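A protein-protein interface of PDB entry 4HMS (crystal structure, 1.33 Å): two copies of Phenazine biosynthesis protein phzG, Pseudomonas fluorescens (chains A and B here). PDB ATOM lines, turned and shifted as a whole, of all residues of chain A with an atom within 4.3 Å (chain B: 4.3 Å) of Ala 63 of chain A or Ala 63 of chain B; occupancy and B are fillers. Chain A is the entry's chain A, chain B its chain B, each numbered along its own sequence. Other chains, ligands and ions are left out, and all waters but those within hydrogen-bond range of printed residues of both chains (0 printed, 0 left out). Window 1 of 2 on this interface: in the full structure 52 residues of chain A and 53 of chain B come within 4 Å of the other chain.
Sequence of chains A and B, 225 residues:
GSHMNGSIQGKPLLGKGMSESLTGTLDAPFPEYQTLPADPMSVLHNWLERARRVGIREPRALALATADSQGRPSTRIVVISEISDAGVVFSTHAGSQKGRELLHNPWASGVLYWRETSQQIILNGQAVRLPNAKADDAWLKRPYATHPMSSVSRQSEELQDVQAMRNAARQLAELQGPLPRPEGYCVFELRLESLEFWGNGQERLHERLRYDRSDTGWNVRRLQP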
ATOM      1  N   ALA A  61      -0.166  -4.675  -2.817  1.00  0.00           N
ATOM      2  CA  ALA A  61      -1.601  -4.749  -3.051  1.00  0.00           C
ATOM      3  C   ALA A  61      -1.965  -6.205  -3.425  1.00  0.00           C
ATOM      4  O   ALA A  61      -1.759  -6.638  -4.560  1.00  0.00           O
ATOM      5  CB  ALA A  61      -2.028  -3.771  -4.129  1.00  0.00           C
ATOM      6  N   LEU A  62      -2.440  -6.949  -2.444  1.00  0.00           N
ATOM      7  CA  LEU A  62      -2.685  -8.380  -2.547  1.00  0.00           C
ATOM      8  C   LEU A  62      -4.155  -8.650  -2.897  1.00  0.00           C
ATOM      9  O   LEU A  62      -5.078  -8.251  -2.158  1.00  0.00           O
ATOM     10  CB  LEU A  62      -2.349  -9.048  -1.201  1.00  0.00           C
ATOM     11  CG  LEU A  62      -2.453 -10.573  -1.142  1.00  0.00           C
ATOM     12  CD1 LEU A  62      -1.334 -11.224  -1.971  1.00  0.00           C
ATOM     13  CD2 LEU A  62      -2.440 -11.074   0.315  1.00  0.00           C
ATOM     14  N   ALA A  63      -4.389  -9.371  -3.988  1.00  0.00           N
ATOM     15  CA  ALA A  63      -5.736  -9.835  -4.332  1.00  0.00           C
ATOM     16  C   ALA A  63      -6.002 -11.117  -3.550  1.00  0.00           C
ATOM     17  O   ALA A  63      -5.478 -12.163  -3.876  1.00  0.00           O
ATOM     18  CB  ALA A  63      -5.850 -10.064  -5.837  1.00  0.00           C
ATOM     19  N   LEU A  64      -6.754 -10.970  -2.452  1.00  0.00           N
ATOM     20  CA  LEU A  64      -6.967 -11.997  -1.439  1.00  0.00           C
ATOM     21  C   LEU A  64      -8.299 -12.727  -1.645  1.00  0.00           C
ATOM     22  O   LEU A  64      -9.353 -12.067  -1.665  1.00  0.00           O
ATOM     23  CB  LEU A  64      -6.961 -11.368  -0.037  1.00  0.00           C
ATOM     24  CG  LEU A  64      -7.189 -12.382   1.102  1.00  0.00           C
ATOM     25  CD1 LEU A  64      -5.992 -13.293   1.339  1.00  0.00           C
ATOM     26  CD2 LEU A  64      -7.576 -11.625   2.378  1.00  0.00           C
ATOM     27  N   ALA A  65      -8.220 -14.042  -1.807  1.00  0.00           N
ATOM     28  CA  ALA A  65      -9.377 -14.899  -1.980  1.00  0.00           C
ATOM     29  C   ALA A  65      -9.643 -15.709  -0.720  1.00  0.00           C
ATOM     30  O   ALA A  65      -8.714 -16.301  -0.123  1.00  0.00           O
ATOM     31  CB  ALA A  65      -9.105 -15.899  -3.119  1.00  0.00           C
ATOM     32  N   ARG A  76     -10.888  -9.517  -3.030  1.00  0.00           N
ATOM     33  CA  ARG A  76     -10.749  -8.060  -2.829  1.00  0.00           C
ATOM     34  C   ARG A  76      -9.278  -7.791  -2.648  1.00  0.00           C
ATOM     35  O   ARG A  76      -8.524  -8.719  -2.358  1.00  0.00           O
ATOM     36  CB  ARG A  76     -11.503  -7.547  -1.582  1.00  0.00           C
ATOM     37  CG  ARG A  76     -10.865  -7.942  -0.254  1.00  0.00           C
ATOM     38  CD  ARG A  76     -10.885  -9.426   0.061  1.00  0.00           C
ATOM     39  NE  ARG A  76     -12.243  -9.925   0.188  1.00  0.00           N
ATOM     40  CZ  ARG A  76     -12.601 -11.190   0.307  1.00  0.00           C
ATOM     41  NH1 ARG A  76     -13.863 -11.470   0.617  1.00  0.00           N
ATOM     42  NH2 ARG A  76     -11.757 -12.186   0.131  1.00  0.00           N
ATOM     43  N   ILE A  77      -8.874  -6.511  -2.777  1.00  0.00           N
ATOM     44  CA  ILE A  77      -7.522  -6.124  -2.469  1.00  0.00           C
ATOM     45  C   ILE A  77      -7.378  -5.843  -0.957  1.00  0.00           C
ATOM     46  O   ILE A  77      -8.179  -5.147  -0.336  1.00  0.00           O
ATOM     47  CB  ILE A  77      -7.111  -4.877  -3.244  1.00  0.00           C
ATOM     48  CG1 ILE A  77      -7.189  -5.111  -4.747  1.00  0.00           C
ATOM     49  CG2 ILE A  77      -5.703  -4.482  -2.856  1.00  0.00           C
ATOM     50  CD1 ILE A  77      -6.260  -6.160  -5.378  1.00  0.00           C
ATOM     51  N   SER A 109      -5.928 -17.678  -0.416  1.00  0.00           N
ATOM     52  CA  SER A 109      -4.872 -17.514  -1.389  1.00  0.00           C
ATOM     53  C   SER A 109      -4.838 -16.075  -1.796  1.00  0.00           C
ATOM     54  O   SER A 109      -5.905 -15.468  -1.901  1.00  0.00           O
ATOM     55  CB  SER A 109      -5.198 -18.396  -2.610  1.00  0.00           C
ATOM     56  OG  SER A 109      -4.204 -18.221  -3.628  1.00  0.00           O
ATOM     57  N   GLY A 110      -3.666 -15.541  -2.102  1.00  0.00           N
ATOM     58  CA  GLY A 110      -3.540 -14.203  -2.627  1.00  0.00           C
ATOM     59  C   GLY A 110      -2.499 -14.128  -3.722  1.00  0.00           C
ATOM     60  O   GLY A 110      -1.500 -14.861  -3.696  1.00  0.00           O
ATOM     61  N   VAL A 111      -2.699 -13.180  -4.638  1.00  0.00           N
ATOM     62  CA  VAL A 111      -1.737 -12.916  -5.685  1.00  0.00           C
ATOM     63  C   VAL A 111      -1.309 -11.453  -5.699  1.00  0.00           C
ATOM     64  O   VAL A 111      -2.146 -10.544  -5.624  1.00  0.00           O
ATOM     65  CB  VAL A 111      -2.231 -13.403  -7.069  1.00  0.00           C
ATOM     66  CG1 VAL A 111      -3.569 -12.797  -7.483  1.00  0.00           C
ATOM     67  CG2 VAL A 111      -1.214 -13.153  -8.174  1.00  0.00           C
ATOM     68  N   ALA B  61      -6.389  -7.233 -16.441  1.00  0.00           N
ATOM     69  CA  ALA B  61      -5.659  -8.253 -15.727  1.00  0.00           C
ATOM     70  C   ALA B  61      -6.419  -8.624 -14.448  1.00  0.00           C
ATOM     71  O   ALA B  61      -6.440  -7.860 -13.456  1.00  0.00           O
ATOM     72  CB  ALA B  61      -4.232  -7.763 -15.401  1.00  0.00           C
ATOM     73  N   LEU B  62      -7.100  -9.759 -14.482  1.00  0.00           N
ATOM     74  CA  LEU B  62      -8.031 -10.216 -13.465  1.00  0.00           C
ATOM     75  C   LEU B  62      -7.379 -11.202 -12.516  1.00  0.00           C
ATOM     76  O   LEU B  62      -6.830 -12.215 -12.957  1.00  0.00           O
ATOM     77  CB  LEU B  62      -9.216 -10.909 -14.178  1.00  0.00           C
ATOM     78  CG  LEU B  62     -10.369 -11.359 -13.277  1.00  0.00           C
ATOM     79  CD1 LEU B  62     -11.116 -10.149 -12.755  1.00  0.00           C
ATOM     80  CD2 LEU B  62     -11.293 -12.322 -14.018  1.00  0.00           C
ATOM     81  N   ALA B  63      -7.362 -10.894 -11.218  1.00  0.00           N
ATOM     82  CA  ALA B  63      -6.856 -11.821 -10.231  1.00  0.00           C
ATOM     83  C   ALA B  63      -8.022 -12.807  -9.957  1.00  0.00           C
ATOM     84  O   ALA B  63      -8.977 -12.472  -9.281  1.00  0.00           O
ATOM     85  CB  ALA B  63      -6.385 -11.122  -8.971  1.00  0.00           C
ATOM     86  N   LEU B  64      -7.927 -14.002 -10.553  1.00  0.00           N
ATOM     87  CA  LEU B  64      -9.020 -14.973 -10.572  1.00  0.00           C
ATOM     88  C   LEU B  64      -8.832 -16.039  -9.502  1.00  0.00           C
ATOM     89  O   LEU B  64      -7.785 -16.745  -9.493  1.00  0.00           O
ATOM     90  CB  LEU B  64      -9.039 -15.655 -11.931  1.00  0.00           C
ATOM     91  CG  LEU B  64     -10.124 -16.737 -12.078  1.00  0.00           C
ATOM     92  CD1 LEU B  64     -11.528 -16.103 -12.122  1.00  0.00           C
ATOM     93  CD2 LEU B  64      -9.877 -17.592 -13.323  1.00  0.00           C
ATOM     94  N   ALA B  65      -9.837 -16.199  -8.653  1.00  0.00           N
ATOM     95  CA  ALA B  65      -9.847 -17.228  -7.614  1.00  0.00           C
ATOM     96  C   ALA B  65     -10.796 -18.359  -7.961  1.00  0.00           C
ATOM     97  O   ALA B  65     -11.939 -18.135  -8.374  1.00  0.00           O
ATOM     98  CB  ALA B  65     -10.332 -16.603  -6.309  1.00  0.00           C
ATOM     99  N   ARG B  76      -4.466 -16.549  -9.430  1.00  0.00           N
ATOM    100  CA  ARG B  76      -3.486 -16.239 -10.492  1.00  0.00           C
ATOM    101  C   ARG B  76      -4.111 -15.146 -11.360  1.00  0.00           C
ATOM    102  O   ARG B  76      -5.319 -14.932 -11.320  1.00  0.00           O
ATOM    103  CB  ARG B  76      -3.168 -17.459 -11.385  1.00  0.00           C
ATOM    104  CG  ARG B  76      -4.276 -17.840 -12.396  1.00  0.00           C
ATOM    105  CD  ARG B  76      -5.568 -18.341 -11.782  1.00  0.00           C
ATOM    106  NE  ARG B  76      -5.317 -19.597 -11.074  1.00  0.00           N
ATOM    107  CZ  ARG B  76      -6.174 -20.221 -10.266  1.00  0.00           C
ATOM    108  NH1 ARG B  76      -5.872 -21.457  -9.855  1.00  0.00           N
ATOM    109  NH2 ARG B  76      -7.320 -19.676  -9.897  1.00  0.00           N
ATOM    110  N   ILE B  77      -3.295 -14.464 -12.148  1.00  0.00           N
ATOM    111  CA  ILE B  77      -3.812 -13.507 -13.127  1.00  0.00           C
ATOM    112  C   ILE B  77      -4.234 -14.213 -14.426  1.00  0.00           C
ATOM    113  O   ILE B  77      -3.492 -15.064 -14.954  1.00  0.00           O
ATOM    114  CB  ILE B  77      -2.731 -12.419 -13.482  1.00  0.00           C
ATOM    115  CG1 ILE B  77      -2.339 -11.605 -12.221  1.00  0.00           C
ATOM    116  CG2 ILE B  77      -3.244 -11.498 -14.582  1.00  0.00           C
ATOM    117  CD1 ILE B  77      -3.458 -10.666 -11.612  1.00  0.00           C
ATOM    118  N   SER B 109     -14.328 -16.139  -8.401  1.00  0.00           N
ATOM    119  CA  SER B 109     -14.386 -14.691  -8.147  1.00  0.00           C
ATOM    120  C   SER B 109     -13.120 -14.091  -8.696  1.00  0.00           C
ATOM    121  O   SER B 109     -12.029 -14.660  -8.499  1.00  0.00           O
ATOM    122  CB  SER B 109     -14.482 -14.432  -6.647  1.00  0.00           C
ATOM    123  OG  SER B 109     -14.472 -13.037  -6.344  1.00  0.00           O
ATOM    124  N   GLY B 110     -13.209 -12.923  -9.307  1.00  0.00           N
ATOM    125  CA  GLY B 110     -12.016 -12.206  -9.720  1.00  0.00           C
ATOM    126  C   GLY B 110     -12.081 -10.735  -9.386  1.00  0.00           C
ATOM    127  O   GLY B 110     -13.159 -10.149  -9.357  1.00  0.00           O
ATOM    128  N   VAL B 111     -10.907 -10.139  -9.206  1.00  0.00           N
ATOM    129  CA  VAL B 111     -10.822  -8.724  -8.903  1.00  0.00           C
ATOM    130  C   VAL B 111      -9.897  -8.006  -9.889  1.00  0.00           C
ATOM    131  O   VAL B 111      -8.779  -8.443 -10.169  1.00  0.00           O
ATOM    132  CB  VAL B 111     -10.399  -8.458  -7.412  1.00  0.00           C
ATOM    133  CG1 VAL B 111      -9.102  -9.132  -6.983  1.00  0.00           C
ATOM    134  CG2 VAL B 111     -10.313  -6.949  -7.114  1.00  0.00           C
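Of chain B, only Ala 63 (3.4 Å) and Val 111 (3.6 Å) come within 4 Å of Ala 63 of chain A.
Ala 63 of chain B touches just these residues of chain A: Ala 63 (3.4 Å) and Val 111 (3.6 Å).
Of the printed residues of chain B, Val 111 of chain A touches Ala 63 (3.6 Å).
Printed residues of chain B within 4 Å of Ala 65 of chain A: Ala 65.
Printed residues of chain A within 4 Å of Ala 65 of chain B: Ala 65 (3.5 Å).
Of the printed residues of chain A, Val 111 of chain B touches Ala 63.
Arg 76 of chain B touches none of the printed residues of chain A.
The nearest printed residue of chain B that does not touch Val 111 of chain A is Arg 76 of chain B (4.3 Å).
CB of Ala 63 of chain A touches CB of Ala 63 of chain B, 3.4 Å away.
Ala 63 of chain A touches Val 111 of chain B.
Ala 65 of chain A touches Ala 65 of chain B.
CB of Ala 63 of chain B touches CG1 of Val 111 of chain A, 3.6 Å away.
Printed residues of chain A that touch a printed residue of chain B: Ala 63, Ala 65 and Val 111.
Hydrophobic or aromatic side chains of chain A within 4 Å of the printed part of chain B: Ala 63, Ala 65 and Val 111.
Of the 10 printed residues of chain B, 3 touch a printed residue of chain A.
Hydrophobic or aromatic side chains of chain B that line the printed part of chain A: Ala 63, Ala 65 and Val 111.
Among the printed residues, 4 pairs touch across the chains.
Among the printed residues, no Asp or Glu carboxylate lies within 4 Å of a Lys or Arg side-chain nitrogen of the other chain.
Ala 63 of chain B touches its own counterpart, Ala 63 of chain A.
Ala 63 of chain A touches Val 111 of chain B, and with the chains exchanged Val 111 of chain A touches Ala 63 of chain B.
Ala 65 of chain B touches its own counterpart, Ala 65 of chain A.
10 positions are printed for both chains.
Of the 4 pairs that touch across the chains among the printed residues, 4 have their exchanged pair printed and touching as well.
The backbone carbonyl oxygen of Val 111 of chain A lies within hydrogen-bond range of the backbone NH of Ala 63 of chain A (3.0 Å).
The backbone NH (N) of Ala 65 of chain A lies within hydrogen-bond range of the backbone carbonyl oxygen (O) of Ser 109 of chain A (2.7 Å).
The backbone NH (N) of Ala 63 of chain B is in hydrogen-bond range of the backbone carbonyl oxygen (O) of Val 111 of chain B, 3.0 Å away.
The backbone NH (N) of Ala 65 of chain B sits at hydrogen-bond distance from the backbone carbonyl oxygen (O) of Ser 109 of chain B (2.7 Å).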
